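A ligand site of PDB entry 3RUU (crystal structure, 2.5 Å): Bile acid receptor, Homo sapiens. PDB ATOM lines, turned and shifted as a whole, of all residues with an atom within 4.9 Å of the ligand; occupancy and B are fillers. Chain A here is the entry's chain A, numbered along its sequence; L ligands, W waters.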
ATOM      1  N   MET A  22      10.148 -20.549  21.129  1.00  0.00           N
ATOM      2  CA  MET A  22      10.429 -19.949  22.432  1.00  0.00           C
ATOM      3  C   MET A  22      10.294 -20.989  23.534  1.00  0.00           C
ATOM      4  O   MET A  22       9.198 -21.504  23.765  1.00  0.00           O
ATOM      5  CB  MET A  22       9.510 -18.753  22.728  1.00  0.00           C
ATOM      6  CG  MET A  22       9.771 -17.505  21.879  1.00  0.00           C
ATOM      7  SD  MET A  22      11.230 -16.543  22.363  1.00  0.00           S
ATOM      8  CE  MET A  22      10.731 -15.895  23.958  1.00  0.00           C
ATOM      9  N   THR A  27      10.253 -18.525  28.826  1.00  0.00           N
ATOM     10  CA  THR A  27       9.063 -17.688  28.917  1.00  0.00           C
ATOM     11  C   THR A  27       8.391 -17.781  30.286  1.00  0.00           C
ATOM     12  O   THR A  27       7.621 -16.888  30.661  1.00  0.00           O
ATOM     13  CB  THR A  27       8.037 -18.019  27.812  1.00  0.00           C
ATOM     14  OG1 THR A  27       7.739 -19.425  27.818  1.00  0.00           O
ATOM     15  CG2 THR A  27       8.604 -17.632  26.448  1.00  0.00           C
ATOM     16  N   ILE A  30       8.573 -14.827  33.005  1.00  0.00           N
ATOM     17  CA  ILE A  30       7.589 -13.754  32.989  1.00  0.00           C
ATOM     18  C   ILE A  30       6.661 -13.898  34.179  1.00  0.00           C
ATOM     19  O   ILE A  30       6.249 -12.907  34.796  1.00  0.00           O
ATOM     20  CB  ILE A  30       6.783 -13.782  31.679  1.00  0.00           C
ATOM     21  CG1 ILE A  30       7.718 -13.581  30.484  1.00  0.00           C
ATOM     22  CG2 ILE A  30       5.669 -12.746  31.701  1.00  0.00           C
ATOM     23  CD1 ILE A  30       7.014 -13.678  29.144  1.00  0.00           C
ATOM     24  N   PHE A  41      13.118  -5.395  33.339  1.00  0.00           N
ATOM     25  CA  PHE A  41      13.948  -5.099  32.185  1.00  0.00           C
ATOM     26  C   PHE A  41      14.774  -6.310  31.756  1.00  0.00           C
ATOM     27  O   PHE A  41      14.916  -6.582  30.570  1.00  0.00           O
ATOM     28  CB  PHE A  41      14.882  -3.918  32.455  1.00  0.00           C
ATOM     29  CG  PHE A  41      15.817  -3.635  31.323  1.00  0.00           C
ATOM     30  CD1 PHE A  41      17.097  -4.168  31.303  1.00  0.00           C
ATOM     31  CD2 PHE A  41      15.394  -2.865  30.245  1.00  0.00           C
ATOM     32  CE1 PHE A  41      17.942  -3.932  30.239  1.00  0.00           C
ATOM     33  CE2 PHE A  41      16.237  -2.619  29.178  1.00  0.00           C
ATOM     34  CZ  PHE A  41      17.523  -3.153  29.179  1.00  0.00           C
ATOM     35  N   LEU A  44      12.537  -8.990  30.010  1.00  0.00           N
ATOM     36  CA  LEU A  44      12.121  -8.553  28.682  1.00  0.00           C
ATOM     37  C   LEU A  44      13.271  -8.637  27.670  1.00  0.00           C
ATOM     38  O   LEU A  44      13.059  -8.919  26.489  1.00  0.00           O
ATOM     39  CB  LEU A  44      11.575  -7.119  28.743  1.00  0.00           C
ATOM     40  CG  LEU A  44      10.257  -6.958  29.492  1.00  0.00           C
ATOM     41  CD1 LEU A  44       9.841  -5.488  29.595  1.00  0.00           C
ATOM     42  CD2 LEU A  44       9.171  -7.805  28.830  1.00  0.00           C
ATOM     43  N   THR A  45      14.486  -8.375  28.144  1.00  0.00           N
ATOM     44  CA  THR A  45      15.686  -8.470  27.317  1.00  0.00           C
ATOM     45  C   THR A  45      15.943  -9.912  26.906  1.00  0.00           C
ATOM     46  O   THR A  45      16.267 -10.202  25.754  1.00  0.00           O
ATOM     47  CB  THR A  45      16.930  -7.924  28.057  1.00  0.00           C
ATOM     48  OG1 THR A  45      16.836  -6.499  28.183  1.00  0.00           O
ATOM     49  CG2 THR A  45      18.190  -8.264  27.298  1.00  0.00           C
ATOM     50  N   MET A  47      13.615 -12.243  26.692  1.00  0.00           N
ATOM     51  CA  MET A  47      12.579 -12.640  25.740  1.00  0.00           C
ATOM     52  C   MET A  47      12.937 -12.153  24.343  1.00  0.00           C
ATOM     53  O   MET A  47      12.924 -12.917  23.370  1.00  0.00           O
ATOM     54  CB  MET A  47      11.211 -12.070  26.147  1.00  0.00           C
ATOM     55  CG  MET A  47      10.756 -12.456  27.536  1.00  0.00           C
ATOM     56  SD  MET A  47      10.582 -14.236  27.747  1.00  0.00           S
ATOM     57  CE  MET A  47      11.575 -14.504  29.205  1.00  0.00           C
ATOM     58  N   ALA A  48      13.274 -10.867  24.229  1.00  0.00           N
ATOM     59  CA  ALA A  48      13.607 -10.275  22.944  1.00  0.00           C
ATOM     60  C   ALA A  48      14.801 -10.955  22.261  1.00  0.00           C
ATOM     61  O   ALA A  48      14.747 -11.260  21.065  1.00  0.00           O
ATOM     62  CB  ALA A  48      13.854  -8.787  23.098  1.00  0.00           C
ATOM     63  N   HIS A  51      13.687 -14.244  21.130  1.00  0.00           N
ATOM     64  CA  HIS A  51      12.728 -14.088  20.038  1.00  0.00           C
ATOM     65  C   HIS A  51      13.422 -13.803  18.711  1.00  0.00           C
ATOM     66  O   HIS A  51      12.992 -14.293  17.660  1.00  0.00           O
ATOM     67  CB  HIS A  51      11.722 -12.973  20.340  1.00  0.00           C
ATOM     68  CG  HIS A  51      10.611 -12.886  19.337  1.00  0.00           C
ATOM     69  ND1 HIS A  51       9.734 -13.927  19.116  1.00  0.00           N
ATOM     70  CD2 HIS A  51      10.245 -11.888  18.502  1.00  0.00           C
ATOM     71  CE1 HIS A  51       8.866 -13.570  18.174  1.00  0.00           C
ATOM     72  NE2 HIS A  51       9.157 -12.338  17.793  1.00  0.00           N
ATOM     73  N   VAL A  82      11.981  -5.334  15.198  1.00  0.00           N
ATOM     74  CA  VAL A  82      11.086  -4.660  16.136  1.00  0.00           C
ATOM     75  C   VAL A  82       9.620  -4.885  15.785  1.00  0.00           C
ATOM     76  O   VAL A  82       8.807  -5.226  16.646  1.00  0.00           O
ATOM     77  CB  VAL A  82      11.364  -3.148  16.184  1.00  0.00           C
ATOM     78  CG1 VAL A  82      10.238  -2.416  16.889  1.00  0.00           C
ATOM     79  CG2 VAL A  82      12.690  -2.884  16.883  1.00  0.00           C
ATOM     80  N   MET A  85       8.440  -8.309  16.700  1.00  0.00           N
ATOM     81  CA  MET A  85       8.234  -8.473  18.138  1.00  0.00           C
ATOM     82  C   MET A  85       6.923  -7.852  18.601  1.00  0.00           C
ATOM     83  O   MET A  85       6.229  -8.403  19.460  1.00  0.00           O
ATOM     84  CB  MET A  85       9.397  -7.874  18.933  1.00  0.00           C
ATOM     85  CG  MET A  85      10.740  -8.527  18.646  1.00  0.00           C
ATOM     86  SD  MET A  85      12.085  -7.769  19.585  1.00  0.00           S
ATOM     87  CE  MET A  85      13.496  -8.504  18.758  1.00  0.00           C
ATOM     88  N   PHE A  86       6.591  -6.688  18.040  1.00  0.00           N
ATOM     89  CA  PHE A  86       5.322  -6.042  18.363  1.00  0.00           C
ATOM     90  C   PHE A  86       4.153  -6.886  17.912  1.00  0.00           C
ATOM     91  O   PHE A  86       3.097  -6.899  18.553  1.00  0.00           O
ATOM     92  CB  PHE A  86       5.227  -4.656  17.719  1.00  0.00           C
ATOM     93  CG  PHE A  86       5.631  -3.536  18.624  1.00  0.00           C
ATOM     94  CD1 PHE A  86       6.910  -2.987  18.558  1.00  0.00           C
ATOM     95  CD2 PHE A  86       4.730  -3.008  19.539  1.00  0.00           C
ATOM     96  CE1 PHE A  86       7.279  -1.941  19.390  1.00  0.00           C
ATOM     97  CE2 PHE A  86       5.100  -1.962  20.371  1.00  0.00           C
ATOM     98  CZ  PHE A  86       6.379  -1.425  20.300  1.00  0.00           C
ATOM     99  N   ARG A  88       4.166 -10.291  17.617  1.00  0.00           N
ATOM    100  CA  ARG A  88       4.094 -11.459  18.488  1.00  0.00           C
ATOM    101  C   ARG A  88       3.594 -11.095  19.879  1.00  0.00           C
ATOM    102  O   ARG A  88       2.721 -11.769  20.434  1.00  0.00           O
ATOM    103  CB  ARG A  88       5.455 -12.150  18.570  1.00  0.00           C
ATOM    104  CG  ARG A  88       5.441 -13.429  19.371  1.00  0.00           C
ATOM    105  CD  ARG A  88       4.412 -14.397  18.865  1.00  0.00           C
ATOM    106  NE  ARG A  88       4.541 -15.707  19.502  1.00  0.00           N
ATOM    107  CZ  ARG A  88       3.782 -16.763  19.236  1.00  0.00           C
ATOM    108  NH1 ARG A  88       2.821 -16.669  18.328  1.00  0.00           N
ATOM    109  NH2 ARG A  88       3.991 -17.902  19.872  1.00  0.00           N
ATOM    110  N   SER A  89       4.120 -10.015  20.449  1.00  0.00           N
ATOM    111  CA  SER A  89       3.617  -9.528  21.729  1.00  0.00           C
ATOM    112  C   SER A  89       2.125  -9.176  21.633  1.00  0.00           C
ATOM    113  O   SER A  89       1.335  -9.547  22.515  1.00  0.00           O
ATOM    114  CB  SER A  89       4.424  -8.322  22.220  1.00  0.00           C
ATOM    115  OG  SER A  89       4.064  -7.143  21.524  1.00  0.00           O
ATOM    116  N   ILE A  92       0.152 -12.216  21.837  1.00  0.00           N
ATOM    117  CA  ILE A  92       0.094 -12.615  23.246  1.00  0.00           C
ATOM    118  C   ILE A  92      -1.071 -11.912  23.936  1.00  0.00           C
ATOM    119  O   ILE A  92      -1.961 -12.560  24.483  1.00  0.00           O
ATOM    120  CB  ILE A  92       1.385 -12.258  24.008  1.00  0.00           C
ATOM    121  CG1 ILE A  92       2.589 -13.041  23.480  1.00  0.00           C
ATOM    122  CG2 ILE A  92       1.200 -12.492  25.507  1.00  0.00           C
ATOM    123  CD1 ILE A  92       2.439 -14.532  23.579  1.00  0.00           C
ATOM    124  N   SER A  99       1.629 -19.417  26.834  1.00  0.00           N
ATOM    125  CA  SER A  99       3.078 -19.211  26.897  1.00  0.00           C
ATOM    126  C   SER A  99       3.483 -17.768  27.178  1.00  0.00           C
ATOM    127  O   SER A  99       4.602 -17.506  27.645  1.00  0.00           O
ATOM    128  CB  SER A  99       3.725 -19.677  25.583  1.00  0.00           C
ATOM    129  N   GLY A 100       2.595 -16.831  26.887  1.00  0.00           N
ATOM    130  CA  GLY A 100       2.910 -15.417  26.996  1.00  0.00           C
ATOM    131  C   GLY A 100       2.633 -14.803  28.360  1.00  0.00           C
ATOM    132  O   GLY A 100       3.270 -13.817  28.745  1.00  0.00           O
ATOM    133  N   LEU A 105       3.134 -10.186  31.696  1.00  0.00           N
ATOM    134  CA  LEU A 105       3.976  -9.601  30.664  1.00  0.00           C
ATOM    135  C   LEU A 105       3.698  -8.099  30.596  1.00  0.00           C
ATOM    136  O   LEU A 105       4.617  -7.288  30.460  1.00  0.00           O
ATOM    137  CB  LEU A 105       3.703 -10.254  29.306  1.00  0.00           C
ATOM    138  CG  LEU A 105       4.575  -9.707  28.154  1.00  0.00           C
ATOM    139  CD1 LEU A 105       6.053  -9.798  28.490  1.00  0.00           C
ATOM    140  CD2 LEU A 105       4.296 -10.395  26.824  1.00  0.00           C
ATOM    141  N   ILE A 109       6.339  -4.906  31.226  1.00  0.00           N
ATOM    142  CA  ILE A 109       6.520  -3.853  30.233  1.00  0.00           C
ATOM    143  C   ILE A 109       6.186  -2.478  30.820  1.00  0.00           C
ATOM    144  O   ILE A 109       6.891  -1.502  30.565  1.00  0.00           O
ATOM    145  CB  ILE A 109       5.657  -4.135  28.980  1.00  0.00           C
ATOM    146  CG1 ILE A 109       6.166  -5.392  28.268  1.00  0.00           C
ATOM    147  CG2 ILE A 109       5.663  -2.920  28.054  1.00  0.00           C
ATOM    148  CD1 ILE A 109       5.325  -5.795  27.088  1.00  0.00           C
ATOM    149  N   ILE A 114      10.206   2.367  30.692  1.00  0.00           N
ATOM    150  CA  ILE A 114       9.680   2.927  29.448  1.00  0.00           C
ATOM    151  C   ILE A 114       8.781   4.131  29.748  1.00  0.00           C
ATOM    152  O   ILE A 114       7.816   4.022  30.496  1.00  0.00           O
ATOM    153  CB  ILE A 114       8.887   1.883  28.650  1.00  0.00           C
ATOM    154  CG1 ILE A 114       9.727   0.626  28.406  1.00  0.00           C
ATOM    155  CG2 ILE A 114       8.397   2.479  27.329  1.00  0.00           C
ATOM    156  CD1 ILE A 114       9.007  -0.459  27.614  1.00  0.00           C
ATOM    157  N   MET A 122       1.857   2.371  22.663  1.00  0.00           N
ATOM    158  CA  MET A 122       2.136   0.944  22.552  1.00  0.00           C
ATOM    159  C   MET A 122       0.895   0.098  22.801  1.00  0.00           C
ATOM    160  O   MET A 122       0.557  -0.770  21.994  1.00  0.00           O
ATOM    161  CB  MET A 122       3.246   0.547  23.540  1.00  0.00           C
ATOM    162  CG  MET A 122       3.546  -0.931  23.593  1.00  0.00           C
ATOM    163  SD  MET A 122       4.910  -1.318  24.713  1.00  0.00           S
ATOM    164  CE  MET A 122       6.118  -0.095  24.199  1.00  0.00           C
ATOM    165  N   TYR A 126      -1.921  -2.288  20.650  1.00  0.00           N
ATOM    166  CA  TYR A 126      -2.333  -3.626  21.087  1.00  0.00           C
ATOM    167  C   TYR A 126      -3.844  -3.811  21.125  1.00  0.00           C
ATOM    168  O   TYR A 126      -4.358  -4.857  20.715  1.00  0.00           O
ATOM    169  CB  TYR A 126      -1.784  -3.915  22.482  1.00  0.00           C
ATOM    170  CG  TYR A 126      -0.296  -4.149  22.537  1.00  0.00           C
ATOM    171  CD1 TYR A 126       0.360  -4.844  21.514  1.00  0.00           C
ATOM    172  CD2 TYR A 126       0.456  -3.704  23.612  1.00  0.00           C
ATOM    173  CE1 TYR A 126       1.722  -5.071  21.575  1.00  0.00           C
ATOM    174  CE2 TYR A 126       1.810  -3.930  23.685  1.00  0.00           C
ATOM    175  CZ  TYR A 126       2.441  -4.610  22.660  1.00  0.00           C
ATOM    176  OH  TYR A 126       3.798  -4.827  22.750  1.00  0.00           O
ATOM    177  N   HIS A 204      11.001   2.980  19.520  1.00  0.00           N
ATOM    178  CA  HIS A 204      11.944   2.002  20.032  1.00  0.00           C
ATOM    179  C   HIS A 204      13.363   2.549  20.100  1.00  0.00           C
ATOM    180  O   HIS A 204      14.102   2.249  21.037  1.00  0.00           O
ATOM    181  CB  HIS A 204      11.880   0.718  19.202  1.00  0.00           C
ATOM    182  CG  HIS A 204      12.579  -0.446  19.837  1.00  0.00           C
ATOM    183  ND1 HIS A 204      13.878  -0.784  19.559  1.00  0.00           N
ATOM    184  CD2 HIS A 204      12.155  -1.330  20.770  1.00  0.00           C
ATOM    185  CE1 HIS A 204      14.225  -1.835  20.277  1.00  0.00           C
ATOM    186  NE2 HIS A 204      13.197  -2.189  21.023  1.00  0.00           N
ATOM    187  N   MET A 207      13.448   4.571  23.177  1.00  0.00           N
ATOM    188  CA  MET A 207      13.408   3.716  24.356  1.00  0.00           C
ATOM    189  C   MET A 207      14.810   3.171  24.632  1.00  0.00           C
ATOM    190  O   MET A 207      15.255   3.108  25.775  1.00  0.00           O
ATOM    191  CB  MET A 207      12.406   2.573  24.179  1.00  0.00           C
ATOM    192  CG  MET A 207      10.948   3.035  24.106  1.00  0.00           C
ATOM    193  SD  MET A 207       9.836   1.795  23.381  1.00  0.00           S
ATOM    194  CE  MET A 207      10.112   0.400  24.476  1.00  0.00           C
ATOM    195  N   TRP A 211      17.137   3.733  28.029  1.00  0.00           N
ATOM    196  CA  TRP A 211      17.692   2.586  28.735  1.00  0.00           C
ATOM    197  C   TRP A 211      19.215   2.709  28.812  1.00  0.00           C
ATOM    198  O   TRP A 211      19.803   2.583  29.882  1.00  0.00           O
ATOM    199  CB  TRP A 211      17.297   1.281  28.034  1.00  0.00           C
ATOM    200  CG  TRP A 211      15.939   0.786  28.410  1.00  0.00           C
ATOM    201  CD1 TRP A 211      15.339   0.871  29.632  1.00  0.00           C
ATOM    202  CD2 TRP A 211      14.987   0.147  27.543  1.00  0.00           C
ATOM    203  NE1 TRP A 211      14.078   0.307  29.591  1.00  0.00           N
ATOM    204  CE2 TRP A 211      13.836  -0.146  28.315  1.00  0.00           C
ATOM    205  CE3 TRP A 211      14.993  -0.224  26.190  1.00  0.00           C
ATOM    206  CZ2 TRP A 211      12.719  -0.778  27.793  1.00  0.00           C
ATOM    207  CZ3 TRP A 211      13.876  -0.856  25.668  1.00  0.00           C
ATOM    208  CH2 TRP A 211      12.757  -1.131  26.460  1.00  0.00           C
ATOM    209  N   PHE A 218      22.096  -4.593  26.854  1.00  0.00           N
ATOM    210  CA  PHE A 218      21.382  -5.591  26.077  1.00  0.00           C
ATOM    211  C   PHE A 218      22.347  -6.715  25.731  1.00  0.00           C
ATOM    212  O   PHE A 218      23.486  -6.737  26.201  1.00  0.00           O
ATOM    213  CB  PHE A 218      20.785  -4.958  24.823  1.00  0.00           C
ATOM    214  CG  PHE A 218      19.929  -3.751  25.126  1.00  0.00           C
ATOM    215  CD1 PHE A 218      20.489  -2.484  25.207  1.00  0.00           C
ATOM    216  CD2 PHE A 218      18.568  -3.893  25.375  1.00  0.00           C
ATOM    217  CE1 PHE A 218      19.708  -1.390  25.504  1.00  0.00           C
ATOM    218  CE2 PHE A 218      17.784  -2.790  25.669  1.00  0.00           C
ATOM    219  CZ  PHE A 218      18.354  -1.538  25.733  1.00  0.00           C
ATOM    220  N   LEU A 222      21.153  -8.535  20.279  1.00  0.00           N
ATOM    221  CA  LEU A 222      20.293  -7.345  20.147  1.00  0.00           C
ATOM    222  C   LEU A 222      21.096  -6.091  19.807  1.00  0.00           C
ATOM    223  O   LEU A 222      20.642  -5.240  19.041  1.00  0.00           O
ATOM    224  CB  LEU A 222      19.489  -7.122  21.429  1.00  0.00           C
ATOM    225  CG  LEU A 222      18.506  -8.227  21.808  1.00  0.00           C
ATOM    226  CD1 LEU A 222      17.916  -7.998  23.186  1.00  0.00           C
ATOM    227  CD2 LEU A 222      17.411  -8.365  20.760  1.00  0.00           C
ATOM    228  N   TRP A 226      20.067  -4.260  16.362  1.00  0.00           N
ATOM    229  CA  TRP A 226      19.515  -2.932  16.639  1.00  0.00           C
ATOM    230  C   TRP A 226      20.550  -1.825  16.505  1.00  0.00           C
ATOM    231  O   TRP A 226      20.240  -0.653  16.647  1.00  0.00           O
ATOM    232  CB  TRP A 226      18.867  -2.879  18.017  1.00  0.00           C
ATOM    233  CG  TRP A 226      17.523  -3.552  18.049  1.00  0.00           C
ATOM    234  CD1 TRP A 226      16.728  -3.841  16.976  1.00  0.00           C
ATOM    235  CD2 TRP A 226      16.830  -4.038  19.211  1.00  0.00           C
ATOM    236  NE1 TRP A 226      15.579  -4.465  17.399  1.00  0.00           N
ATOM    237  CE2 TRP A 226      15.619  -4.593  18.758  1.00  0.00           C
ATOM    238  CE3 TRP A 226      17.121  -4.049  20.578  1.00  0.00           C
ATOM    239  CZ2 TRP A 226      14.689  -5.159  19.629  1.00  0.00           C
ATOM    240  CZ3 TRP A 226      16.201  -4.613  21.446  1.00  0.00           C
ATOM    241  CH2 TRP A 226      14.991  -5.157  20.965  1.00  0.00           C
HETATM  242  C1  LIG L   1       9.554 -10.801  22.580  1.00  0.00           C
HETATM  243  C2  LIG L   1       8.359 -10.245  24.584  1.00  0.00           C
HETATM  244  C3  LIG L   1       8.013 -12.474  23.472  1.00  0.00           C
HETATM  245  C4  LIG L   1       6.895 -15.024  23.350  1.00  0.00           C
HETATM  246  C5  LIG L   1       6.290 -16.231  23.593  1.00  0.00           C
HETATM  247  C6  LIG L   1       6.018 -16.278  24.956  1.00  0.00           C
HETATM  248  C7  LIG L   1       6.968 -14.347  24.563  1.00  0.00           C
HETATM  249  C8  LIG L   1       5.998 -17.294  22.601  1.00  0.00           C
HETATM  250  C9  LIG L   1      15.061  -5.761  24.986  1.00  0.00           C
HETATM  251  C10 LIG L   1      13.748  -5.573  25.656  1.00  0.00           C
HETATM  252  C11 LIG L   1      13.865  -4.977  27.054  1.00  0.00           C
HETATM  253  C12 LIG L   1      12.724  -4.858  24.777  1.00  0.00           C
HETATM  254  O1  LIG L   1      12.927  -3.641  24.206  1.00  0.00           O
HETATM  255  N1  LIG L   1      11.795  -3.312  23.486  1.00  0.00           N
HETATM  256  C13 LIG L   1      10.900  -4.317  23.595  1.00  0.00           C
HETATM  257  C14 LIG L   1      11.454  -5.290  24.400  1.00  0.00           C
HETATM  258  C15 LIG L   1      10.733  -6.641  24.771  1.00  0.00           C
HETATM  259  O2  LIG L   1      10.551  -7.476  23.614  1.00  0.00           O
HETATM  260  C16 LIG L   1       9.914  -8.674  23.625  1.00  0.00           C
HETATM  261  C17 LIG L   1      10.187  -9.572  22.622  1.00  0.00           C
HETATM  262  C18 LIG L   1       8.643 -11.143  23.546  1.00  0.00           C
HETATM  263  C19 LIG L   1       8.987  -9.011  24.614  1.00  0.00           C
HETATM  264  C20 LIG L   1       7.948 -13.157  22.238  1.00  0.00           C
HETATM  265  C21 LIG L   1       7.385 -14.422  22.191  1.00  0.00           C
HETATM  266  N2  LIG L   1       6.431 -15.127  25.512  1.00  0.00           N
HETATM  267  C22 LIG L   1       7.525 -13.088  24.626  1.00  0.00           C
HETATM  268  O3  LIG L   1       6.159 -17.078  21.357  1.00  0.00           O
HETATM  269  O4  LIG L   1       5.575 -18.495  23.023  1.00  0.00           O
HETATM  270  C23 LIG L   1       9.557  -4.367  22.969  1.00  0.00           C
HETATM  271  C24 LIG L   1       8.441  -4.104  23.728  1.00  0.00           C
HETATM  272 CL1  LIG L   1       8.596  -3.715  25.390  1.00  0.00          CL
HETATM  273  C25 LIG L   1       7.175  -4.152  23.155  1.00  0.00           C
HETATM  274  C26 LIG L   1       7.050  -4.465  21.797  1.00  0.00           C
HETATM  275  C27 LIG L   1       8.165  -4.732  21.029  1.00  0.00           C
HETATM  276  C28 LIG L   1       9.423  -4.682  21.613  1.00  0.00           C
HETATM  277 CL2  LIG L   1      10.793  -5.013  20.678  1.00  0.00          CL
HETATM  278  O   HOH W   1       7.175 -20.042  25.238  1.00  0.00           O
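NH2 of Arg 88 lies within salt-bridge range of O3 of the ligand, at 2.8 Å.
A ring nitrogen (NE2) of His 204 is in hydrogen-bond range of a nitrogen (N1) of the ligand, 3.0 Å away.
O of Met 85 is in hydrogen-bond range of OG of Ser 89 (3.2 Å).
O of Phe 86 lies within hydrogen-bond range of OG of Ser 89, 3.1 Å away.
The side-chain hydroxyl (OH) of Tyr 126 lies within hydrogen-bond range of the side-chain hydroxyl (OG) of Ser 89, at 2.6 Å.
O of Phe 41 is in hydrogen-bond range of OG1 of Thr 45 (3.1 Å).
SD of Met 22 is in hydrogen-bond range of N of His 51 (3.6 Å).
Merely in contact with the ligand: Met 22 (3.7 Å), Thr 27 (3.3 Å), Ile 30 (3.95 Å), Phe 41 (3.96 Å), Leu 44 (3.5 Å), Thr 45 (3.5 Å), Met 47 (3.7 Å), Ala 48 (3.5 Å), His 51 (3.7 Å), Met 85 (3.2 Å), Phe 86 (3.3 Å), Ser 99 (3.3 Å), Gly 100 (3.8 Å), Ile 114 (3.96 Å), Met 122 (3.9 Å), Tyr 126 (3.4 Å), Trp 211 (3.3 Å), Phe 218 (3.99 Å) and Trp 226 (3.9 Å).
Water W1 lies within hydrogen-bond range of the side-chain hydroxyl of Thr 27 (2.7 Å), the backbone carbonyl oxygen of Met 22 (2.9 Å) and an oxygen (O4) of the ligand (3.1 Å).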
